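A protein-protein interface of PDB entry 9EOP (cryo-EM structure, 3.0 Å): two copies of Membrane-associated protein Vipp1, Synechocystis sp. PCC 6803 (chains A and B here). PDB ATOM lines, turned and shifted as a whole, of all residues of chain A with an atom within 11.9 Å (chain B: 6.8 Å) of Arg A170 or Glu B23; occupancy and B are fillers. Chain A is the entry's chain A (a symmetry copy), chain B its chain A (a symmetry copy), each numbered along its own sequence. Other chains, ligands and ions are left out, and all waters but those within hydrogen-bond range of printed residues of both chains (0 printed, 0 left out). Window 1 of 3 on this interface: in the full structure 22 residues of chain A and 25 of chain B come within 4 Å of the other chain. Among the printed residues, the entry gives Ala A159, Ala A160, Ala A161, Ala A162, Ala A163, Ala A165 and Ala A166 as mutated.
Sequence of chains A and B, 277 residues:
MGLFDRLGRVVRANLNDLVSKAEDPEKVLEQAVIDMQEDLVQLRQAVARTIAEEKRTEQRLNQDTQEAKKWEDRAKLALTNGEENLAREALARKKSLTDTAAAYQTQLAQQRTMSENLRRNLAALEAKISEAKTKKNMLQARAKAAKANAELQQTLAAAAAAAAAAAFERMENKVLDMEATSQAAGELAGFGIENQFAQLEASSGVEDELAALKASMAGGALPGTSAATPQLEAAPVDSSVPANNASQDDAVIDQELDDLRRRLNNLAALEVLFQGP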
ATOM      1  N   ALA A 159      10.773  -3.149 -13.508  1.00  0.00           N
ATOM      2  CA  ALA A 159       9.687  -3.218 -12.540  1.00  0.00           C
ATOM      3  C   ALA A 159       8.433  -2.512 -13.032  1.00  0.00           C
ATOM      4  O   ALA A 159       7.317  -2.999 -12.819  1.00  0.00           O
ATOM      5  CB  ALA A 159      10.139  -2.605 -11.223  1.00  0.00           C
ATOM      6  N   ALA A 160       8.592  -1.367 -13.687  1.00  0.00           N
ATOM      7  CA  ALA A 160       7.443  -0.667 -14.244  1.00  0.00           C
ATOM      8  C   ALA A 160       6.828  -1.404 -15.424  1.00  0.00           C
ATOM      9  O   ALA A 160       5.636  -1.233 -15.702  1.00  0.00           O
ATOM     10  CB  ALA A 160       7.856   0.736 -14.667  1.00  0.00           C
ATOM     11  N   ALA A 161       7.612  -2.213 -16.131  1.00  0.00           N
ATOM     12  CA  ALA A 161       7.052  -2.992 -17.228  1.00  0.00           C
ATOM     13  C   ALA A 161       6.191  -4.154 -16.749  1.00  0.00           C
ATOM     14  O   ALA A 161       5.302  -4.598 -17.483  1.00  0.00           O
ATOM     15  CB  ALA A 161       8.175  -3.518 -18.111  1.00  0.00           C
ATOM     16  N   ALA A 162       6.434  -4.669 -15.545  1.00  0.00           N
ATOM     17  CA  ALA A 162       5.602  -5.757 -15.045  1.00  0.00           C
ATOM     18  C   ALA A 162       4.242  -5.279 -14.550  1.00  0.00           C
ATOM     19  O   ALA A 162       3.245  -5.988 -14.717  1.00  0.00           O
ATOM     20  CB  ALA A 162       6.333  -6.489 -13.926  1.00  0.00           C
ATOM     21  N   ALA A 163       4.178  -4.093 -13.956  1.00  0.00           N
ATOM     22  CA  ALA A 163       2.920  -3.476 -13.548  1.00  0.00           C
ATOM     23  C   ALA A 163       2.065  -4.437 -12.725  1.00  0.00           C
ATOM     24  O   ALA A 163       0.884  -4.655 -12.998  1.00  0.00           O
ATOM     25  CB  ALA A 163       2.156  -2.982 -14.768  1.00  0.00           C
ATOM     26  N   ALA A 164       2.689  -5.027 -11.710  1.00  0.00           N
ATOM     27  CA  ALA A 164       1.974  -5.881 -10.773  1.00  0.00           C
ATOM     28  C   ALA A 164       0.832  -5.153 -10.075  1.00  0.00           C
ATOM     29  O   ALA A 164      -0.196  -5.759  -9.759  1.00  0.00           O
ATOM     30  CB  ALA A 164       2.953  -6.429  -9.748  1.00  0.00           C
ATOM     31  N   ALA A 165       0.997  -3.857  -9.828  1.00  0.00           N
ATOM     32  CA  ALA A 165      -0.054  -3.039  -9.234  1.00  0.00           C
ATOM     33  C   ALA A 165      -1.276  -2.892 -10.127  1.00  0.00           C
ATOM     34  O   ALA A 165      -2.397  -2.773  -9.619  1.00  0.00           O
ATOM     35  CB  ALA A 165       0.501  -1.666  -8.891  1.00  0.00           C
ATOM     36  N   ALA A 166      -1.092  -2.884 -11.441  1.00  0.00           N
ATOM     37  CA  ALA A 166      -2.224  -2.860 -12.355  1.00  0.00           C
ATOM     38  C   ALA A 166      -2.933  -4.203 -12.448  1.00  0.00           C
ATOM     39  O   ALA A 166      -4.162  -4.250 -12.560  1.00  0.00           O
ATOM     40  CB  ALA A 166      -1.747  -2.438 -13.733  1.00  0.00           C
ATOM     41  N   ALA A 167      -2.185  -5.298 -12.409  1.00  0.00           N
ATOM     42  CA  ALA A 167      -2.805  -6.614 -12.347  1.00  0.00           C
ATOM     43  C   ALA A 167      -3.655  -6.772 -11.098  1.00  0.00           C
ATOM     44  O   ALA A 167      -4.724  -7.389 -11.138  1.00  0.00           O
ATOM     45  CB  ALA A 167      -1.732  -7.690 -12.397  1.00  0.00           C
ATOM     46  N   PHE A 168      -3.197  -6.222  -9.980  1.00  0.00           N
ATOM     47  CA  PHE A 168      -3.985  -6.254  -8.756  1.00  0.00           C
ATOM     48  C   PHE A 168      -5.276  -5.460  -8.897  1.00  0.00           C
ATOM     49  O   PHE A 168      -6.356  -5.937  -8.532  1.00  0.00           O
ATOM     50  CB  PHE A 168      -3.130  -5.690  -7.626  1.00  0.00           C
ATOM     51  CG  PHE A 168      -3.678  -5.921  -6.263  1.00  0.00           C
ATOM     52  CD1 PHE A 168      -4.606  -5.061  -5.721  1.00  0.00           C
ATOM     53  CD2 PHE A 168      -3.239  -6.978  -5.504  1.00  0.00           C
ATOM     54  CE1 PHE A 168      -5.096  -5.271  -4.464  1.00  0.00           C
ATOM     55  CE2 PHE A 168      -3.729  -7.187  -4.253  1.00  0.00           C
ATOM     56  CZ  PHE A 168      -4.656  -6.333  -3.730  1.00  0.00           C
ATOM     57  N   GLU A 169      -5.183  -4.247  -9.429  1.00  0.00           N
ATOM     58  CA  GLU A 169      -6.369  -3.431  -9.664  1.00  0.00           C
ATOM     59  C   GLU A 169      -7.323  -4.071 -10.661  1.00  0.00           C
ATOM     60  O   GLU A 169      -8.545  -4.013 -10.493  1.00  0.00           O
ATOM     61  CB  GLU A 169      -5.944  -2.056 -10.152  1.00  0.00           C
ATOM     62  CG  GLU A 169      -7.087  -1.110 -10.400  1.00  0.00           C
ATOM     63  CD  GLU A 169      -6.625   0.222 -10.951  1.00  0.00           C
ATOM     64  OE1 GLU A 169      -5.908   0.222 -11.974  1.00  0.00           O
ATOM     65  OE2 GLU A 169      -6.973   1.266 -10.362  1.00  0.00           O
ATOM     66  N   ARG A 170      -6.782  -4.679 -11.712  1.00  0.00           N
ATOM     67  CA  ARG A 170      -7.604  -5.360 -12.702  1.00  0.00           C
ATOM     68  C   ARG A 170      -8.296  -6.595 -12.146  1.00  0.00           C
ATOM     69  O   ARG A 170      -9.417  -6.912 -12.558  1.00  0.00           O
ATOM     70  CB  ARG A 170      -6.729  -5.730 -13.893  1.00  0.00           C
ATOM     71  CG  ARG A 170      -7.438  -6.434 -14.993  1.00  0.00           C
ATOM     72  CD  ARG A 170      -6.601  -6.481 -16.249  1.00  0.00           C
ATOM     73  NE  ARG A 170      -5.321  -7.157 -16.074  1.00  0.00           N
ATOM     74  CZ  ARG A 170      -4.141  -6.554 -16.050  1.00  0.00           C
ATOM     75  NH1 ARG A 170      -4.030  -5.240 -16.110  1.00  0.00           N
ATOM     76  NH2 ARG A 170      -3.040  -7.290 -15.978  1.00  0.00           N
ATOM     77  N   MET A 171      -7.654  -7.304 -11.231  1.00  0.00           N
ATOM     78  CA  MET A 171      -8.217  -8.517 -10.658  1.00  0.00           C
ATOM     79  C   MET A 171      -9.152  -8.269  -9.488  1.00  0.00           C
ATOM     80  O   MET A 171      -9.989  -9.124  -9.188  1.00  0.00           O
ATOM     81  CB  MET A 171      -7.089  -9.444 -10.242  1.00  0.00           C
ATOM     82  CG  MET A 171      -7.417 -10.876 -10.427  1.00  0.00           C
ATOM     83  SD  MET A 171      -7.831 -11.350 -12.106  1.00  0.00           S
ATOM     84  CE  MET A 171      -6.319 -10.937 -12.911  1.00  0.00           C
ATOM     85  N   GLU A 172      -9.032  -7.128  -8.823  1.00  0.00           N
ATOM     86  CA  GLU A 172     -10.037  -6.726  -7.853  1.00  0.00           C
ATOM     87  C   GLU A 172     -11.405  -6.541  -8.494  1.00  0.00           C
ATOM     88  O   GLU A 172     -12.427  -6.922  -7.916  1.00  0.00           O
ATOM     89  CB  GLU A 172      -9.590  -5.437  -7.180  1.00  0.00           C
ATOM     90  CG  GLU A 172     -10.623  -4.800  -6.302  1.00  0.00           C
ATOM     91  CD  GLU A 172     -10.099  -3.574  -5.593  1.00  0.00           C
ATOM     92  OE1 GLU A 172      -8.898  -3.272  -5.740  1.00  0.00           O
ATOM     93  OE2 GLU A 172     -10.887  -2.913  -4.887  1.00  0.00           O
ATOM     94  N   ASN A 173     -11.443  -5.948  -9.681  1.00  0.00           N
ATOM     95  CA  ASN A 173     -12.711  -5.673 -10.339  1.00  0.00           C
ATOM     96  C   ASN A 173     -13.464  -6.929 -10.755  1.00  0.00           C
ATOM     97  O   ASN A 173     -14.698  -6.928 -10.762  1.00  0.00           O
ATOM     98  CB  ASN A 173     -12.444  -4.805 -11.555  1.00  0.00           C
ATOM     99  CG  ASN A 173     -12.129  -3.379 -11.189  1.00  0.00           C
ATOM    100  OD1 ASN A 173     -12.178  -2.998 -10.022  1.00  0.00           O
ATOM    101  ND2 ASN A 173     -11.772  -2.590 -12.182  1.00  0.00           N
ATOM    102  N   LYS A 174     -12.761  -8.002 -11.111  1.00  0.00           N
ATOM    103  CA  LYS A 174     -13.430  -9.270 -11.378  1.00  0.00           C
ATOM    104  C   LYS A 174     -14.133  -9.832 -10.153  1.00  0.00           C
ATOM    105  O   LYS A 174     -15.234 -10.383 -10.257  1.00  0.00           O
ATOM    106  CB  LYS A 174     -12.426 -10.286 -11.888  1.00  0.00           C
ATOM    107  CG  LYS A 174     -11.928 -10.037 -13.264  1.00  0.00           C
ATOM    108  CD  LYS A 174     -11.272 -11.278 -13.792  1.00  0.00           C
ATOM    109  CE  LYS A 174     -10.767 -11.099 -15.191  1.00  0.00           C
ATOM    110  NZ  LYS A 174     -10.261 -12.384 -15.720  1.00  0.00           N
ATOM    111  N   VAL A 175     -13.509  -9.714  -8.988  1.00  0.00           N
ATOM    112  CA  VAL A 175     -14.109 -10.208  -7.757  1.00  0.00           C
ATOM    113  C   VAL A 175     -15.408  -9.485  -7.451  1.00  0.00           C
ATOM    114  O   VAL A 175     -16.401 -10.096  -7.043  1.00  0.00           O
ATOM    115  CB  VAL A 175     -13.102 -10.058  -6.607  1.00  0.00           C
ATOM    116  CG1 VAL A 175     -13.727 -10.406  -5.296  1.00  0.00           C
ATOM    117  CG2 VAL A 175     -11.913 -10.925  -6.860  1.00  0.00           C
ATOM    118  N   LEU A 176     -15.418  -8.177  -7.643  1.00  0.00           N
ATOM    119  CA  LEU A 176     -16.607  -7.381  -7.394  1.00  0.00           C
ATOM    120  C   LEU A 176     -17.725  -7.676  -8.381  1.00  0.00           C
ATOM    121  O   LEU A 176     -18.902  -7.540  -8.034  1.00  0.00           O
ATOM    122  CB  LEU A 176     -16.214  -5.918  -7.433  1.00  0.00           C
ATOM    123  CG  LEU A 176     -15.838  -5.340  -6.078  1.00  0.00           C
ATOM    124  CD1 LEU A 176     -14.749  -6.134  -5.494  1.00  0.00           C
ATOM    125  CD2 LEU A 176     -15.356  -3.947  -6.232  1.00  0.00           C
ATOM    126  N   ASP A 177     -17.387  -8.068  -9.604  1.00  0.00           N
ATOM    127  CA  ASP A 177     -18.406  -8.498 -10.554  1.00  0.00           C
ATOM    128  C   ASP A 177     -19.010  -9.851 -10.198  1.00  0.00           C
ATOM    129  O   ASP A 177     -20.218 -10.055 -10.362  1.00  0.00           O
ATOM    130  CB  ASP A 177     -17.798  -8.555 -11.947  1.00  0.00           C
ATOM    131  CG  ASP A 177     -17.461  -7.188 -12.493  1.00  0.00           C
ATOM    132  OD1 ASP A 177     -17.809  -6.184 -11.842  1.00  0.00           O
ATOM    133  OD2 ASP A 177     -16.848  -7.117 -13.577  1.00  0.00           O
ATOM    134  N   MET A 178     -18.199 -10.786  -9.711  1.00  0.00           N
ATOM    135  CA  MET A 178     -18.724 -12.058  -9.226  1.00  0.00           C
ATOM    136  C   MET A 178     -19.661 -11.871  -8.045  1.00  0.00           C
ATOM    137  O   MET A 178     -20.754 -12.446  -7.999  1.00  0.00           O
ATOM    138  CB  MET A 178     -17.575 -12.978  -8.838  1.00  0.00           C
ATOM    139  CG  MET A 178     -16.710 -13.406  -9.984  1.00  0.00           C
ATOM    140  SD  MET A 178     -15.234 -14.275  -9.422  1.00  0.00           S
ATOM    141  CE  MET A 178     -14.354 -14.463 -10.969  1.00  0.00           C
ATOM    142  N   LEU B  18      -8.181 -12.023 -24.946  1.00  0.00           N
ATOM    143  CA  LEU B  18      -8.115 -13.474 -24.839  1.00  0.00           C
ATOM    144  C   LEU B  18      -7.225 -13.926 -23.689  1.00  0.00           C
ATOM    145  O   LEU B  18      -7.540 -14.896 -22.992  1.00  0.00           O
ATOM    146  CB  LEU B  18      -7.604 -14.030 -26.159  1.00  0.00           C
ATOM    147  CG  LEU B  18      -7.545 -15.529 -26.353  1.00  0.00           C
ATOM    148  CD1 LEU B  18      -8.944 -16.047 -26.509  1.00  0.00           C
ATOM    149  CD2 LEU B  18      -6.723 -15.829 -27.568  1.00  0.00           C
ATOM    150  N   VAL B  19      -6.109 -13.237 -23.478  1.00  0.00           N
ATOM    151  CA  VAL B  19      -5.279 -13.465 -22.299  1.00  0.00           C
ATOM    152  C   VAL B  19      -5.990 -13.041 -21.020  1.00  0.00           C
ATOM    153  O   VAL B  19      -5.966 -13.759 -20.016  1.00  0.00           O
ATOM    154  CB  VAL B  19      -3.942 -12.724 -22.455  1.00  0.00           C
ATOM    155  CG1 VAL B  19      -3.164 -12.738 -21.169  1.00  0.00           C
ATOM    156  CG2 VAL B  19      -3.136 -13.338 -23.561  1.00  0.00           C
ATOM    157  N   SER B  20      -6.624 -11.875 -21.031  1.00  0.00           N
ATOM    158  CA  SER B  20      -7.172 -11.320 -19.799  1.00  0.00           C
ATOM    159  C   SER B  20      -8.210 -12.218 -19.142  1.00  0.00           C
ATOM    160  O   SER B  20      -8.305 -12.241 -17.912  1.00  0.00           O
ATOM    161  CB  SER B  20      -7.788  -9.956 -20.077  1.00  0.00           C
ATOM    162  OG  SER B  20      -8.258  -9.371 -18.880  1.00  0.00           O
ATOM    163  N   LYS B  21      -8.997 -12.953 -19.915  1.00  0.00           N
ATOM    164  CA  LYS B  21      -9.955 -13.878 -19.325  1.00  0.00           C
ATOM    165  C   LYS B  21      -9.364 -15.243 -19.002  1.00  0.00           C
ATOM    166  O   LYS B  21     -10.103 -16.137 -18.580  1.00  0.00           O
ATOM    167  CB  LYS B  21     -11.156 -14.047 -20.252  1.00  0.00           C
ATOM    168  CG  LYS B  21     -10.855 -14.797 -21.510  1.00  0.00           C
ATOM    169  CD  LYS B  21     -11.900 -14.492 -22.559  1.00  0.00           C
ATOM    170  CE  LYS B  21     -11.559 -15.138 -23.882  1.00  0.00           C
ATOM    171  NZ  LYS B  21     -12.226 -14.460 -25.024  1.00  0.00           N
ATOM    172  N   ALA B  22      -8.064 -15.426 -19.190  1.00  0.00           N
ATOM    173  CA  ALA B  22      -7.364 -16.591 -18.669  1.00  0.00           C
ATOM    174  C   ALA B  22      -6.870 -16.410 -17.242  1.00  0.00           C
ATOM    175  O   ALA B  22      -6.546 -17.402 -16.582  1.00  0.00           O
ATOM    176  CB  ALA B  22      -6.171 -16.930 -19.556  1.00  0.00           C
ATOM    177  N   GLU B  23      -6.795 -15.176 -16.760  1.00  0.00           N
ATOM    178  CA  GLU B  23      -6.342 -14.906 -15.404  1.00  0.00           C
ATOM    179  C   GLU B  23      -7.394 -15.300 -14.372  1.00  0.00           C
ATOM    180  O   GLU B  23      -8.493 -14.735 -14.344  1.00  0.00           O
ATOM    181  CB  GLU B  23      -5.993 -13.427 -15.296  1.00  0.00           C
ATOM    182  CG  GLU B  23      -4.847 -13.030 -16.208  1.00  0.00           C
ATOM    183  CD  GLU B  23      -4.374 -11.601 -16.023  1.00  0.00           C
ATOM    184  OE1 GLU B  23      -5.158 -10.759 -15.549  1.00  0.00           O
ATOM    185  OE2 GLU B  23      -3.205 -11.318 -16.353  1.00  0.00           O
ATOM    186  N   ASP B  24      -7.049 -16.268 -13.527  1.00  0.00           N
ATOM    187  CA  ASP B  24      -7.879 -16.649 -12.388  1.00  0.00           C
ATOM    188  C   ASP B  24      -7.656 -15.687 -11.226  1.00  0.00           C
ATOM    189  O   ASP B  24      -6.530 -15.588 -10.729  1.00  0.00           O
ATOM    190  CB  ASP B  24      -7.567 -18.067 -11.948  1.00  0.00           C
ATOM    191  CG  ASP B  24      -8.439 -18.527 -10.801  1.00  0.00           C
ATOM    192  OD1 ASP B  24      -9.354 -17.777 -10.404  1.00  0.00           O
ATOM    193  OD2 ASP B  24      -8.211 -19.643 -10.291  1.00  0.00           O
ATOM    194  N   PRO B  25      -8.679 -14.965 -10.772  1.00  0.00           N
ATOM    195  CA  PRO B  25      -8.450 -13.941  -9.743  1.00  0.00           C
ATOM    196  C   PRO B  25      -7.736 -14.428  -8.499  1.00  0.00           C
ATOM    197  O   PRO B  25      -6.781 -13.798  -8.034  1.00  0.00           O
ATOM    198  CB  PRO B  25      -9.870 -13.475  -9.416  1.00  0.00           C
ATOM    199  CG  PRO B  25     -10.635 -13.729 -10.608  1.00  0.00           C
ATOM    200  CD  PRO B  25     -10.079 -14.973 -11.210  1.00  0.00           C
ATOM    201  N   GLU B  26      -8.182 -15.549  -7.949  1.00  0.00           N
ATOM    202  CA  GLU B  26      -7.720 -15.986  -6.642  1.00  0.00           C
ATOM    203  C   GLU B  26      -6.248 -16.367  -6.650  1.00  0.00           C
ATOM    204  O   GLU B  26      -5.549 -16.161  -5.653  1.00  0.00           O
ATOM    205  CB  GLU B  26      -8.576 -17.157  -6.178  1.00  0.00           C
ATOM    206  CG  GLU B  26      -8.581 -17.360  -4.685  1.00  0.00           C
ATOM    207  CD  GLU B  26      -9.501 -18.480  -4.251  1.00  0.00           C
ATOM    208  OE1 GLU B  26     -10.450 -18.793  -4.999  1.00  0.00           O
ATOM    209  OE2 GLU B  26      -9.275 -19.043  -3.160  1.00  0.00           O
ATOM    210  N   VAL B  28      -3.876 -15.254  -9.206  1.00  0.00           N
ATOM    211  CA  VAL B  28      -3.032 -14.169  -9.682  1.00  0.00           C
ATOM    212  C   VAL B  28      -3.025 -13.007  -8.710  1.00  0.00           C
ATOM    213  O   VAL B  28      -2.066 -12.229  -8.662  1.00  0.00           O
ATOM    214  CB  VAL B  28      -3.517 -13.718 -11.067  1.00  0.00           C
ATOM    215  CG1 VAL B  28      -2.708 -12.562 -11.562  1.00  0.00           C
ATOM    216  CG2 VAL B  28      -3.453 -14.850 -12.040  1.00  0.00           C
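NZ of Lys A174 is in hydrogen-bond range of O of Ser B20, at 2.9 Å. The side-chain carboxylate of Glu B23 lies within salt-bridge range of the guanidinium group of Arg A170 (3.6 Å). The side-chain amino group (NZ) of Lys A174 lies within hydrogen-bond range of the backbone carbonyl oxygen (O) of Glu B23.
CE of Met A171 touches OE1 of Glu B23, at 2.9 Å. CA of Pro B25 touches CG of Met A171, at 3.3 Å. Lys B21 touches Lys A174. Pro B25 touches Met A178 (CG to CE, 3.8 Å).
Arg A170 touches one residue of chain B. Of the printed residues of chain A, Glu B23 touches Arg A170, Met A171 and Lys A174. No residue of chain A comes within 4 Å of Val B19. Ser B20 touches just one residue of chain A: Lys A174 (2.9 Å). No residue of chain A comes within 4 Å of Asp B24. Pro B25 touches just these residues of chain A: Met A171 and Met A178. Printed residues of chain B within 4 Å of Met A178: Pro B25. Of the printed residues of chain A, Lys B21 touches Lys A174. Of the printed residues of chain B, Lys A174 touches Ser B20 (2.9 Å), Lys B21 (3.9 Å) and Glu B23 (3.2 Å). Ala A164 touches none of the printed residues of chain B. Val A175 touches none of the printed residues of chain B. The nearest residue of chain A that does not touch Glu B23 is Ala A167 (5.6 Å).
Of the 20 printed residues of chain A, 4 touch a printed residue of chain B. Printed residues of chain A that touch a printed residue of chain B: Arg A170, Met A171, Lys A174 and Met A178. Of the 10 printed residues of chain B, 4 touch a printed residue of chain A. Printed residues of chain B that touch a printed residue of chain A: Ser B20, Lys B21, Glu B23 and Pro B25. Hydrophobic or aromatic side chains of chain B that line the printed part of chain A: Pro B25.
No position is printed for both chains. Of the 7 pairs that touch across the chains among the printed residues, none has its exchanged pair printed and touching as well.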
